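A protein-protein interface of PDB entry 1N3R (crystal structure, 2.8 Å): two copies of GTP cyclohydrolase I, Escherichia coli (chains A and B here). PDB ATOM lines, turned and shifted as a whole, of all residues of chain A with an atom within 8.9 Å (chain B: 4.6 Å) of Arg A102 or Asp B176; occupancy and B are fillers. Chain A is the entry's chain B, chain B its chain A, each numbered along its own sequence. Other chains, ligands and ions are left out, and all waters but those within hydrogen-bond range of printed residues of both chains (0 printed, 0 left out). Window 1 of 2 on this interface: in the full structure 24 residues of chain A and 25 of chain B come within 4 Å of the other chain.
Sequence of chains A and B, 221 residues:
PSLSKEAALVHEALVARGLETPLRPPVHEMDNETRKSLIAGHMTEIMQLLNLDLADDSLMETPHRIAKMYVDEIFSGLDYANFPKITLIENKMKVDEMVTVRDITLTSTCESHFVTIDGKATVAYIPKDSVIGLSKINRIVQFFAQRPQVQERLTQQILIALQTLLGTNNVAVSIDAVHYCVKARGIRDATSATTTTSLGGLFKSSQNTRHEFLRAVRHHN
Printed residues of chain B within 4 Å of Val A99: Thr B195. Of the printed residues of chain B, Thr A100 touches Ala B193 (3.9 Å), Thr B194 (3.3 Å) and Thr B195 (2.7 Å). Of chain B, only Asp B176 (2.6 Å), Ser B192 (3.1 Å), Ala B193 (3.0 Å), Thr B195 (3.7 Å) and Arg B218 (2.5 Å) come within 4 Å of Arg A102. Printed residues of chain B within 4 Å of Thr A105: Thr B191 (2.9 Å). Ser A174 touches none of the printed residues of chain B. Ala A216 touches none of the printed residues of chain B. Printed residues of chain B within 4 Å of Asn A221: Arg B218 and His B220. No residue of chain A comes within 4 Å of Gly B119. Of chain A, only Arg A102 comes within 4 Å of Asp B176. No residue of chain A comes within 4 Å of Ala B177. Of chain A, only Thr A100, Val A101 and Arg A102 come within 4 Å of Ala B193.
Positions printed for both chains: 120, 174, 218 and 220.
Of the 14 printed residues of chain B, 8 touch a printed residue of chain A. Hydrophobic or aromatic side chains of chain B within 4 Å of the printed part of chain A: Ala B193 and His B220. Of the 25 printed residues of chain A, 11 touch a printed residue of chain B. Printed residues of chain A that touch a printed residue of chain B: Val A99, Thr A100, Val A101, Arg A102, Asp A103, Thr A105, Lys A120, Leu A134, Asn A138, His A219 and Asn A221. Among the printed residues, 20 pairs touch across the chains.
O of Asp B176 is in hydrogen-bond range of N of Lys B120 (2.9 Å). N of Ala B177 is in hydrogen-bond range of O of Thr B194, at 2.8 Å. NH1 of Arg B218 lies within hydrogen-bond range of ND1 of His B220. NH1 of Arg A102 lies within salt-bridge range of OD2 of Asp A103 (2.6 Å). NE2 of His A219 lies close to O of Ala A216 (3.1 Å). A ring nitrogen (ND1) of His A220 lies close to the side-chain amide oxygen (OD1) of Asn A221 (2.9 Å).
The side-chain carboxylate (OD2) of Asp B176 is in salt-bridge range of the guanidinium group (NH2) of Arg A102, at 2.6 Å. The side-chain hydroxyl (OG1) of Thr B191 sits at hydrogen-bond distance from the backbone carbonyl oxygen (O) of Asp A103. The side-chain hydroxyl of Thr A105 sits at hydrogen-bond distance from the side-chain hydroxyl of Thr B191, at 2.9 Å. N of Ser B192 lies within hydrogen-bond range of O of Asp A103, 3.0 Å away. OG of Ser B192 lies within hydrogen-bond range of OD1 of Asn A138 (3.2 Å). The backbone carbonyl oxygen (O) of Ala B193 lies within hydrogen-bond range of the backbone NH (N) of Arg A102. The backbone NH (N) of Thr B195 lies within hydrogen-bond range of the backbone carbonyl oxygen (O) of Thr A100 (2.7 Å). The guanidinium group of Arg A102 sits close to the guanidinium group of Arg B218, 2.5 Å away. The guanidinium group of Arg B218 lies within hydrogen-bond range of the backbone carbonyl oxygen of Asn A221 (2.4 Å).
Val A99 touches Thr B195. CA of Thr B194 touches O of Thr A100, at 3.3 Å. Val A101 touches Ala B193. Val A101 touches Thr B194. O of Arg A102 touches CB of Ser B192 (3.1 Å). NE of Arg A102 touches OG1 of Thr B195, 3.7 Å away. Lys A120 touches Thr B191 (CE to OG1, 3.7 Å). Thr B194 touches Leu A134 (OG1 to CD1, 3.5 Å). Arg B218 touches His A219 (CG to CE1, 3.3 Å). Asn A221 touches His B220 (C to CE1, 3.9 Å).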
ATOM      1  N   VAL A  99       5.120 -36.882 -31.523  1.00  0.00           N
ATOM      2  CA  VAL A  99       5.260 -36.001 -30.370  1.00  0.00           C
ATOM      3  C   VAL A  99       6.498 -35.138 -30.648  1.00  0.00           C
ATOM      4  O   VAL A  99       7.616 -35.642 -30.834  1.00  0.00           O
ATOM      5  CB  VAL A  99       5.427 -36.810 -29.053  1.00  0.00           C
ATOM      6  CG1 VAL A  99       5.734 -35.885 -27.910  1.00  0.00           C
ATOM      7  CG2 VAL A  99       4.149 -37.564 -28.742  1.00  0.00           C
ATOM      8  N   THR A 100       6.276 -33.829 -30.654  1.00  0.00           N
ATOM      9  CA  THR A 100       7.309 -32.855 -30.962  1.00  0.00           C
ATOM     10  C   THR A 100       7.751 -31.932 -29.823  1.00  0.00           C
ATOM     11  O   THR A 100       6.928 -31.410 -29.067  1.00  0.00           O
ATOM     12  CB  THR A 100       6.822 -31.986 -32.109  1.00  0.00           C
ATOM     13  OG1 THR A 100       6.079 -32.806 -33.018  1.00  0.00           O
ATOM     14  CG2 THR A 100       7.990 -31.342 -32.827  1.00  0.00           C
ATOM     15  N   VAL A 101       9.059 -31.730 -29.721  1.00  0.00           N
ATOM     16  CA  VAL A 101       9.618 -30.842 -28.713  1.00  0.00           C
ATOM     17  C   VAL A 101      10.512 -29.864 -29.472  1.00  0.00           C
ATOM     18  O   VAL A 101      11.576 -30.228 -29.974  1.00  0.00           O
ATOM     19  CB  VAL A 101      10.434 -31.629 -27.651  1.00  0.00           C
ATOM     20  CG1 VAL A 101      11.053 -30.683 -26.638  1.00  0.00           C
ATOM     21  CG2 VAL A 101       9.523 -32.601 -26.935  1.00  0.00           C
ATOM     22  N   ARG A 102      10.062 -28.620 -29.562  1.00  0.00           N
ATOM     23  CA  ARG A 102      10.806 -27.594 -30.277  1.00  0.00           C
ATOM     24  C   ARG A 102      11.578 -26.605 -29.403  1.00  0.00           C
ATOM     25  O   ARG A 102      11.530 -26.653 -28.175  1.00  0.00           O
ATOM     26  CB  ARG A 102       9.854 -26.827 -31.191  1.00  0.00           C
ATOM     27  CG  ARG A 102       8.670 -26.272 -30.458  1.00  0.00           C
ATOM     28  CD  ARG A 102       7.600 -25.818 -31.423  1.00  0.00           C
ATOM     29  NE  ARG A 102       6.457 -25.244 -30.721  1.00  0.00           N
ATOM     30  CZ  ARG A 102       6.513 -24.134 -29.991  1.00  0.00           C
ATOM     31  NH1 ARG A 102       7.660 -23.480 -29.873  1.00  0.00           N
ATOM     32  NH2 ARG A 102       5.433 -23.681 -29.371  1.00  0.00           N
ATOM     33  N   ASP A 103      12.298 -25.710 -30.077  1.00  0.00           N
ATOM     34  CA  ASP A 103      13.112 -24.677 -29.448  1.00  0.00           C
ATOM     35  C   ASP A 103      13.897 -25.163 -28.241  1.00  0.00           C
ATOM     36  O   ASP A 103      13.890 -24.534 -27.184  1.00  0.00           O
ATOM     37  CB  ASP A 103      12.246 -23.482 -29.062  1.00  0.00           C
ATOM     38  CG  ASP A 103      11.366 -23.023 -30.201  1.00  0.00           C
ATOM     39  OD1 ASP A 103      11.862 -22.961 -31.343  1.00  0.00           O
ATOM     40  OD2 ASP A 103      10.177 -22.726 -29.961  1.00  0.00           O
ATOM     41  N   ILE A 104      14.570 -26.291 -28.405  1.00  0.00           N
ATOM     42  CA  ILE A 104      15.376 -26.847 -27.340  1.00  0.00           C
ATOM     43  C   ILE A 104      16.725 -26.123 -27.280  1.00  0.00           C
ATOM     44  O   ILE A 104      17.498 -26.101 -28.241  1.00  0.00           O
ATOM     45  CB  ILE A 104      15.596 -28.355 -27.550  1.00  0.00           C
ATOM     46  CG1 ILE A 104      14.251 -29.083 -27.494  1.00  0.00           C
ATOM     47  CG2 ILE A 104      16.545 -28.897 -26.503  1.00  0.00           C
ATOM     48  CD1 ILE A 104      14.326 -30.531 -27.930  1.00  0.00           C
ATOM     49  N   THR A 105      16.978 -25.519 -26.129  1.00  0.00           N
ATOM     50  CA  THR A 105      18.206 -24.795 -25.854  1.00  0.00           C
ATOM     51  C   THR A 105      19.408 -25.700 -26.084  1.00  0.00           C
ATOM     52  O   THR A 105      19.642 -26.628 -25.322  1.00  0.00           O
ATOM     53  CB  THR A 105      18.206 -24.321 -24.389  1.00  0.00           C
ATOM     54  OG1 THR A 105      17.127 -23.399 -24.192  1.00  0.00           O
ATOM     55  CG2 THR A 105      19.508 -23.670 -24.026  1.00  0.00           C
ATOM     56  N   LEU A 106      20.150 -25.446 -27.154  1.00  0.00           N
ATOM     57  CA  LEU A 106      21.337 -26.232 -27.453  1.00  0.00           C
ATOM     58  C   LEU A 106      22.535 -25.315 -27.386  1.00  0.00           C
ATOM     59  O   LEU A 106      22.625 -24.328 -28.122  1.00  0.00           O
ATOM     60  CB  LEU A 106      21.247 -26.863 -28.842  1.00  0.00           C
ATOM     61  CG  LEU A 106      22.455 -27.664 -29.352  1.00  0.00           C
ATOM     62  CD1 LEU A 106      21.965 -28.764 -30.290  1.00  0.00           C
ATOM     63  CD2 LEU A 106      23.482 -26.720 -30.025  1.00  0.00           C
ATOM     64  N   LYS A 120      19.263 -24.079 -31.423  1.00  0.00           N
ATOM     65  CA  LYS A 120      17.935 -24.512 -30.987  1.00  0.00           C
ATOM     66  C   LYS A 120      17.562 -25.772 -31.762  1.00  0.00           C
ATOM     67  O   LYS A 120      17.474 -25.758 -32.988  1.00  0.00           O
ATOM     68  CB  LYS A 120      16.892 -23.436 -31.277  1.00  0.00           C
ATOM     69  CG  LYS A 120      16.359 -22.701 -30.062  1.00  0.00           C
ATOM     70  CD  LYS A 120      17.341 -21.671 -29.549  1.00  0.00           C
ATOM     71  CE  LYS A 120      16.698 -20.827 -28.461  1.00  0.00           C
ATOM     72  NZ  LYS A 120      15.338 -20.316 -28.852  1.00  0.00           N
ATOM     73  N   ALA A 121      17.322 -26.863 -31.052  1.00  0.00           N
ATOM     74  CA  ALA A 121      16.991 -28.112 -31.724  1.00  0.00           C
ATOM     75  C   ALA A 121      15.520 -28.434 -31.653  1.00  0.00           C
ATOM     76  O   ALA A 121      14.852 -28.068 -30.701  1.00  0.00           O
ATOM     77  CB  ALA A 121      17.796 -29.253 -31.122  1.00  0.00           C
ATOM     78  N   THR A 122      15.012 -29.096 -32.681  1.00  0.00           N
ATOM     79  CA  THR A 122      13.616 -29.504 -32.707  1.00  0.00           C
ATOM     80  C   THR A 122      13.635 -31.025 -32.873  1.00  0.00           C
ATOM     81  O   THR A 122      14.325 -31.553 -33.745  1.00  0.00           O
ATOM     82  CB  THR A 122      12.872 -28.847 -33.858  1.00  0.00           C
ATOM     83  OG1 THR A 122      13.028 -27.428 -33.760  1.00  0.00           O
ATOM     84  CG2 THR A 122      11.388 -29.210 -33.803  1.00  0.00           C
ATOM     85  N   VAL A 123      12.899 -31.721 -32.018  1.00  0.00           N
ATOM     86  CA  VAL A 123      12.888 -33.172 -32.040  1.00  0.00           C
ATOM     87  C   VAL A 123      11.496 -33.734 -32.102  1.00  0.00           C
ATOM     88  O   VAL A 123      10.580 -33.226 -31.452  1.00  0.00           O
ATOM     89  CB  VAL A 123      13.612 -33.729 -30.799  1.00  0.00           C
ATOM     90  CG1 VAL A 123      13.309 -35.197 -30.605  1.00  0.00           C
ATOM     91  CG2 VAL A 123      15.104 -33.514 -30.957  1.00  0.00           C
ATOM     92  N   ALA A 124      11.361 -34.810 -32.873  1.00  0.00           N
ATOM     93  CA  ALA A 124      10.083 -35.486 -33.065  1.00  0.00           C
ATOM     94  C   ALA A 124      10.241 -37.004 -33.182  1.00  0.00           C
ATOM     95  O   ALA A 124      11.225 -37.499 -33.725  1.00  0.00           O
ATOM     96  CB  ALA A 124       9.385 -34.925 -34.321  1.00  0.00           C
ATOM     97  N   LEU A 134       9.512 -36.315 -21.268  1.00  0.00           N
ATOM     98  CA  LEU A 134       9.794 -35.142 -22.081  1.00  0.00           C
ATOM     99  C   LEU A 134      11.142 -34.453 -21.853  1.00  0.00           C
ATOM    100  O   LEU A 134      11.906 -34.268 -22.793  1.00  0.00           O
ATOM    101  CB  LEU A 134       8.649 -34.135 -21.946  1.00  0.00           C
ATOM    102  CG  LEU A 134       7.355 -34.438 -22.722  1.00  0.00           C
ATOM    103  CD1 LEU A 134       6.364 -33.310 -22.507  1.00  0.00           C
ATOM    104  CD2 LEU A 134       7.637 -34.637 -24.193  1.00  0.00           C
ATOM    105  N   ILE A 137      14.411 -35.762 -23.439  1.00  0.00           N
ATOM    106  CA  ILE A 137      14.777 -35.416 -24.799  1.00  0.00           C
ATOM    107  C   ILE A 137      15.697 -34.187 -24.745  1.00  0.00           C
ATOM    108  O   ILE A 137      16.783 -34.167 -25.327  1.00  0.00           O
ATOM    109  CB  ILE A 137      13.525 -35.095 -25.631  1.00  0.00           C
ATOM    110  CG1 ILE A 137      12.646 -36.339 -25.733  1.00  0.00           C
ATOM    111  CG2 ILE A 137      13.932 -34.591 -27.021  1.00  0.00           C
ATOM    112  CD1 ILE A 137      11.321 -36.092 -26.461  1.00  0.00           C
ATOM    113  N   ASN A 138      15.258 -33.166 -24.024  1.00  0.00           N
ATOM    114  CA  ASN A 138      16.045 -31.958 -23.884  1.00  0.00           C
ATOM    115  C   ASN A 138      17.435 -32.323 -23.360  1.00  0.00           C
ATOM    116  O   ASN A 138      18.457 -31.789 -23.823  1.00  0.00           O
ATOM    117  CB  ASN A 138      15.376 -31.019 -22.883  1.00  0.00           C
ATOM    118  CG  ASN A 138      14.013 -30.545 -23.336  1.00  0.00           C
ATOM    119  OD1 ASN A 138      13.836 -29.365 -23.606  1.00  0.00           O
ATOM    120  ND2 ASN A 138      13.039 -31.451 -23.404  1.00  0.00           N
ATOM    121  N   VAL A 141      19.756 -34.075 -26.037  1.00  0.00           N
ATOM    122  CA  VAL A 141      20.202 -33.083 -26.990  1.00  0.00           C
ATOM    123  C   VAL A 141      21.418 -32.399 -26.357  1.00  0.00           C
ATOM    124  O   VAL A 141      22.496 -32.311 -26.954  1.00  0.00           O
ATOM    125  CB  VAL A 141      19.109 -32.022 -27.255  1.00  0.00           C
ATOM    126  CG1 VAL A 141      19.671 -30.897 -28.137  1.00  0.00           C
ATOM    127  CG2 VAL A 141      17.892 -32.676 -27.909  1.00  0.00           C
ATOM    128  N   SER A 174      16.132 -31.863 -35.894  1.00  0.00           N
ATOM    129  CA  SER A 174      16.515 -30.666 -36.657  1.00  0.00           C
ATOM    130  C   SER A 174      17.262 -29.680 -35.746  1.00  0.00           C
ATOM    131  O   SER A 174      16.908 -29.513 -34.579  1.00  0.00           O
ATOM    132  CB  SER A 174      15.260 -30.009 -37.244  1.00  0.00           C
ATOM    133  OG  SER A 174      15.569 -28.941 -38.129  1.00  0.00           O
ATOM    134  N   PHE A 213       6.588 -32.743 -40.386  1.00  0.00           N
ATOM    135  CA  PHE A 213       7.643 -32.409 -39.440  1.00  0.00           C
ATOM    136  C   PHE A 213       8.349 -31.140 -39.898  1.00  0.00           C
ATOM    137  O   PHE A 213       8.437 -30.163 -39.155  1.00  0.00           O
ATOM    138  CB  PHE A 213       8.675 -33.534 -39.350  1.00  0.00           C
ATOM    139  CG  PHE A 213       9.915 -33.159 -38.580  1.00  0.00           C
ATOM    140  CD1 PHE A 213       9.876 -33.018 -37.198  1.00  0.00           C
ATOM    141  CD2 PHE A 213      11.118 -32.924 -39.247  1.00  0.00           C
ATOM    142  CE1 PHE A 213      11.018 -32.651 -36.491  1.00  0.00           C
ATOM    143  CE2 PHE A 213      12.265 -32.555 -38.554  1.00  0.00           C
ATOM    144  CZ  PHE A 213      12.218 -32.416 -37.172  1.00  0.00           C
ATOM    145  N   ALA A 216       6.612 -28.009 -39.463  1.00  0.00           N
ATOM    146  CA  ALA A 216       6.516 -27.595 -38.067  1.00  0.00           C
ATOM    147  C   ALA A 216       7.866 -27.224 -37.463  1.00  0.00           C
ATOM    148  O   ALA A 216       7.943 -26.823 -36.304  1.00  0.00           O
ATOM    149  CB  ALA A 216       5.861 -28.692 -37.244  1.00  0.00           C
ATOM    150  N   VAL A 217       8.928 -27.355 -38.246  1.00  0.00           N
ATOM    151  CA  VAL A 217      10.259 -27.020 -37.761  1.00  0.00           C
ATOM    152  C   VAL A 217      10.498 -25.524 -37.911  1.00  0.00           C
ATOM    153  O   VAL A 217       9.855 -24.862 -38.727  1.00  0.00           O
ATOM    154  CB  VAL A 217      11.350 -27.785 -38.541  1.00  0.00           C
ATOM    155  CG1 VAL A 217      12.730 -27.336 -38.085  1.00  0.00           C
ATOM    156  CG2 VAL A 217      11.180 -29.287 -38.339  1.00  0.00           C
ATOM    157  N   ARG A 218      11.417 -24.999 -37.107  1.00  0.00           N
ATOM    158  CA  ARG A 218      11.777 -23.583 -37.124  1.00  0.00           C
ATOM    159  C   ARG A 218      10.656 -22.680 -36.592  1.00  0.00           C
ATOM    160  O   ARG A 218       9.707 -22.352 -37.311  1.00  0.00           O
ATOM    161  CB  ARG A 218      12.180 -23.156 -38.546  1.00  0.00           C
ATOM    162  CG  ARG A 218      13.296 -22.110 -38.613  1.00  0.00           C
ATOM    163  CD  ARG A 218      12.877 -20.796 -37.974  1.00  0.00           C
ATOM    164  NE  ARG A 218      13.919 -19.775 -38.022  1.00  0.00           N
ATOM    165  CZ  ARG A 218      13.861 -18.635 -37.339  1.00  0.00           C
ATOM    166  NH1 ARG A 218      12.814 -18.385 -36.563  1.00  0.00           N
ATOM    167  NH2 ARG A 218      14.844 -17.750 -37.425  1.00  0.00           N
ATOM    168  N   HIS A 219      10.787 -22.285 -35.324  1.00  0.00           N
ATOM    169  CA  HIS A 219       9.826 -21.400 -34.654  1.00  0.00           C
ATOM    170  C   HIS A 219      10.512 -20.445 -33.670  1.00  0.00           C
ATOM    171  O   HIS A 219      11.588 -20.738 -33.142  1.00  0.00           O
ATOM    172  CB  HIS A 219       8.751 -22.215 -33.917  1.00  0.00           C
ATOM    173  CG  HIS A 219       7.741 -22.843 -34.827  1.00  0.00           C
ATOM    174  ND1 HIS A 219       7.043 -22.125 -35.775  1.00  0.00           N
ATOM    175  CD2 HIS A 219       7.318 -24.124 -34.941  1.00  0.00           C
ATOM    176  CE1 HIS A 219       6.236 -22.937 -36.436  1.00  0.00           C
ATOM    177  NE2 HIS A 219       6.384 -24.156 -35.950  1.00  0.00           N
ATOM    178  N   HIS A 220       9.886 -19.291 -33.448  1.00  0.00           N
ATOM    179  CA  HIS A 220      10.414 -18.281 -32.533  1.00  0.00           C
ATOM    180  C   HIS A 220       9.394 -18.021 -31.424  1.00  0.00           C
ATOM    181  O   HIS A 220       8.270 -17.579 -31.692  1.00  0.00           O
ATOM    182  CB  HIS A 220      10.706 -16.980 -33.289  1.00  0.00           C
ATOM    183  CG  HIS A 220      11.412 -15.948 -32.462  1.00  0.00           C
ATOM    184  ND1 HIS A 220      10.934 -15.511 -31.247  1.00  0.00           N
ATOM    185  CD2 HIS A 220      12.556 -15.257 -32.685  1.00  0.00           C
ATOM    186  CE1 HIS A 220      11.750 -14.596 -30.756  1.00  0.00           C
ATOM    187  NE2 HIS A 220      12.742 -14.423 -31.609  1.00  0.00           N
ATOM    188  N   ASN A 221       9.796 -18.292 -30.182  1.00  0.00           N
ATOM    189  CA  ASN A 221       8.930 -18.118 -29.018  1.00  0.00           C
ATOM    190  C   ASN A 221       7.628 -18.897 -29.167  1.00  0.00           C
ATOM    191  O   ASN A 221       7.532 -19.801 -29.996  1.00  0.00           O
ATOM    192  CB  ASN A 221       8.622 -16.634 -28.778  1.00  0.00           C
ATOM    193  CG  ASN A 221       9.712 -15.932 -27.992  1.00  0.00           C
ATOM    194  OD1 ASN A 221      10.881 -15.961 -28.370  1.00  0.00           O
ATOM    195  ND2 ASN A 221       9.331 -15.301 -26.887  1.00  0.00           N
ATOM    196  N   ASP B 118       1.546 -25.076 -18.881  1.00  0.00           N
ATOM    197  CA  ASP B 118       0.824 -23.955 -19.471  1.00  0.00           C
ATOM    198  C   ASP B 118       0.774 -24.140 -20.972  1.00  0.00           C
ATOM    199  O   ASP B 118       1.827 -24.256 -21.601  1.00  0.00           O
ATOM    200  CB  ASP B 118       1.535 -22.649 -19.135  1.00  0.00           C
ATOM    201  CG  ASP B 118       0.731 -21.432 -19.525  1.00  0.00           C
ATOM    202  OD1 ASP B 118      -0.424 -21.309 -19.041  1.00  0.00           O
ATOM    203  OD2 ASP B 118       1.262 -20.609 -20.308  1.00  0.00           O
ATOM    204  N   GLY B 119      -0.435 -24.161 -21.539  1.00  0.00           N
ATOM    205  CA  GLY B 119      -0.560 -24.354 -22.972  1.00  0.00           C
ATOM    206  C   GLY B 119      -1.716 -23.728 -23.734  1.00  0.00           C
ATOM    207  O   GLY B 119      -2.575 -23.021 -23.204  1.00  0.00           O
ATOM    208  N   LYS B 120      -1.700 -23.989 -25.034  1.00  0.00           N
ATOM    209  CA  LYS B 120      -2.713 -23.506 -25.953  1.00  0.00           C
ATOM    210  C   LYS B 120      -3.158 -24.719 -26.729  1.00  0.00           C
ATOM    211  O   LYS B 120      -2.319 -25.546 -27.107  1.00  0.00           O
ATOM    212  CB  LYS B 120      -2.115 -22.474 -26.910  1.00  0.00           C
ATOM    213  CG  LYS B 120      -2.457 -21.044 -26.549  1.00  0.00           C
ATOM    214  CD  LYS B 120      -1.647 -20.554 -25.374  1.00  0.00           C
ATOM    215  CE  LYS B 120      -2.476 -19.614 -24.547  1.00  0.00           C
ATOM    216  NZ  LYS B 120      -3.481 -18.918 -25.397  1.00  0.00           N
ATOM    217  N   SER B 174      -4.968 -30.613 -30.860  1.00  0.00           N
ATOM    218  CA  SER B 174      -3.535 -30.356 -30.902  1.00  0.00           C
ATOM    219  C   SER B 174      -3.228 -29.518 -29.682  1.00  0.00           C
ATOM    220  O   SER B 174      -4.024 -28.648 -29.332  1.00  0.00           O
ATOM    221  CB  SER B 174      -3.191 -29.587 -32.199  1.00  0.00           C
ATOM    222  OG  SER B 174      -1.801 -29.381 -32.375  1.00  0.00           O
ATOM    223  N   ILE B 175      -2.112 -29.786 -29.008  1.00  0.00           N
ATOM    224  CA  ILE B 175      -1.772 -28.997 -27.825  1.00  0.00           C
ATOM    225  C   ILE B 175      -0.308 -28.624 -27.783  1.00  0.00           C
ATOM    226  O   ILE B 175       0.576 -29.488 -27.840  1.00  0.00           O
ATOM    227  CB  ILE B 175      -2.126 -29.726 -26.487  1.00  0.00           C
ATOM    228  CG1 ILE B 175      -3.630 -30.052 -26.435  1.00  0.00           C
ATOM    229  CG2 ILE B 175      -1.718 -28.854 -25.297  1.00  0.00           C
ATOM    230  CD1 ILE B 175      -4.060 -30.775 -25.174  1.00  0.00           C
ATOM    231  N   ASP B 176      -0.070 -27.319 -27.682  1.00  0.00           N
ATOM    232  CA  ASP B 176       1.276 -26.784 -27.606  1.00  0.00           C
ATOM    233  C   ASP B 176       1.426 -26.265 -26.200  1.00  0.00           C
ATOM    234  O   ASP B 176       0.684 -25.364 -25.797  1.00  0.00           O
ATOM    235  CB  ASP B 176       1.462 -25.634 -28.576  1.00  0.00           C
ATOM    236  CG  ASP B 176       2.899 -25.187 -28.640  1.00  0.00           C
ATOM    237  OD1 ASP B 176       3.672 -25.864 -29.351  1.00  0.00           O
ATOM    238  OD2 ASP B 176       3.261 -24.195 -27.963  1.00  0.00           O
ATOM    239  N   ALA B 177       2.390 -26.805 -25.459  1.00  0.00           N
ATOM    240  CA  ALA B 177       2.565 -26.405 -24.063  1.00  0.00           C
ATOM    241  C   ALA B 177       3.983 -26.290 -23.520  1.00  0.00           C
ATOM    242  O   ALA B 177       4.921 -26.916 -24.009  1.00  0.00           O
ATOM    243  CB  ALA B 177       1.772 -27.363 -23.161  1.00  0.00           C
ATOM    244  N   THR B 191      13.374 -22.223 -23.148  1.00  0.00           N
ATOM    245  CA  THR B 191      12.938 -21.866 -24.497  1.00  0.00           C
ATOM    246  C   THR B 191      12.091 -22.933 -25.213  1.00  0.00           C
ATOM    247  O   THR B 191      11.403 -22.625 -26.182  1.00  0.00           O
ATOM    248  CB  THR B 191      14.173 -21.506 -25.386  1.00  0.00           C
ATOM    249  OG1 THR B 191      14.810 -22.704 -25.843  1.00  0.00           O
ATOM    250  CG2 THR B 191      15.216 -20.739 -24.581  1.00  0.00           C
ATOM    251  N   SER B 192      12.117 -24.177 -24.739  1.00  0.00           N
ATOM    252  CA  SER B 192      11.359 -25.244 -25.409  1.00  0.00           C
ATOM    253  C   SER B 192       9.870 -25.335 -25.109  1.00  0.00           C
ATOM    254  O   SER B 192       9.366 -24.744 -24.151  1.00  0.00           O
ATOM    255  CB  SER B 192      11.973 -26.605 -25.117  1.00  0.00           C
ATOM    256  OG  SER B 192      11.596 -27.070 -23.833  1.00  0.00           O
ATOM    257  N   ALA B 193       9.170 -26.094 -25.942  1.00  0.00           N
ATOM    258  CA  ALA B 193       7.738 -26.302 -25.788  1.00  0.00           C
ATOM    259  C   ALA B 193       7.402 -27.630 -26.453  1.00  0.00           C
ATOM    260  O   ALA B 193       8.125 -28.086 -27.351  1.00  0.00           O
ATOM    261  CB  ALA B 193       6.973 -25.193 -26.432  1.00  0.00           C
ATOM    262  N   THR B 194       6.311 -28.252 -26.018  1.00  0.00           N
ATOM    263  CA  THR B 194       5.934 -29.539 -26.563  1.00  0.00           C
ATOM    264  C   THR B 194       4.640 -29.458 -27.311  1.00  0.00           C
ATOM    265  O   THR B 194       3.718 -28.766 -26.894  1.00  0.00           O
ATOM    266  CB  THR B 194       5.809 -30.582 -25.453  1.00  0.00           C
ATOM    267  OG1 THR B 194       7.047 -30.641 -24.729  1.00  0.00           O
ATOM    268  CG2 THR B 194       5.509 -31.962 -26.041  1.00  0.00           C
ATOM    269  N   THR B 195       4.573 -30.179 -28.422  1.00  0.00           N
ATOM    270  CA  THR B 195       3.375 -30.185 -29.238  1.00  0.00           C
ATOM    271  C   THR B 195       2.921 -31.622 -29.430  1.00  0.00           C
ATOM    272  O   THR B 195       3.693 -32.463 -29.863  1.00  0.00           O
ATOM    273  CB  THR B 195       3.652 -29.524 -30.612  1.00  0.00           C
ATOM    274  OG1 THR B 195       4.397 -28.318 -30.404  1.00  0.00           O
ATOM    275  CG2 THR B 195       2.341 -29.176 -31.331  1.00  0.00           C
ATOM    276  N   ARG B 218       0.194 -22.658 -34.766  1.00  0.00           N
ATOM    277  CA  ARG B 218       1.317 -21.886 -34.201  1.00  0.00           C
ATOM    278  C   ARG B 218       1.009 -20.431 -33.812  1.00  0.00           C
ATOM    279  O   ARG B 218       1.210 -19.495 -34.588  1.00  0.00           O
ATOM    280  CB  ARG B 218       2.579 -21.935 -35.075  1.00  0.00           C
ATOM    281  CG  ARG B 218       3.871 -22.051 -34.238  1.00  0.00           C
ATOM    282  CD  ARG B 218       3.985 -20.940 -33.178  1.00  0.00           C
ATOM    283  NE  ARG B 218       4.912 -21.260 -32.090  1.00  0.00           N
ATOM    284  CZ  ARG B 218       4.722 -20.886 -30.825  1.00  0.00           C
ATOM    285  NH1 ARG B 218       3.646 -20.181 -30.498  1.00  0.00           N
ATOM    286  NH2 ARG B 218       5.585 -21.231 -29.879  1.00  0.00           N
ATOM    287  N   HIS B 220       0.542 -18.350 -29.609  1.00  0.00           N
ATOM    288  CA  HIS B 220       0.456 -18.460 -28.149  1.00  0.00           C
ATOM    289  C   HIS B 220       1.315 -17.362 -27.474  1.00  0.00           C
ATOM    290  O   HIS B 220       1.406 -16.248 -27.994  1.00  0.00           O
ATOM    291  CB  HIS B 220       0.805 -19.896 -27.680  1.00  0.00           C
ATOM    292  CG  HIS B 220       2.232 -20.140 -27.294  1.00  0.00           C
ATOM    293  ND1 HIS B 220       3.245 -19.243 -27.537  1.00  0.00           N
ATOM    294  CD2 HIS B 220       2.817 -21.199 -26.677  1.00  0.00           C
ATOM    295  CE1 HIS B 220       4.389 -19.730 -27.087  1.00  0.00           C
ATOM    296  NE2 HIS B 220       4.157 -20.915 -26.560  1.00  0.00           N
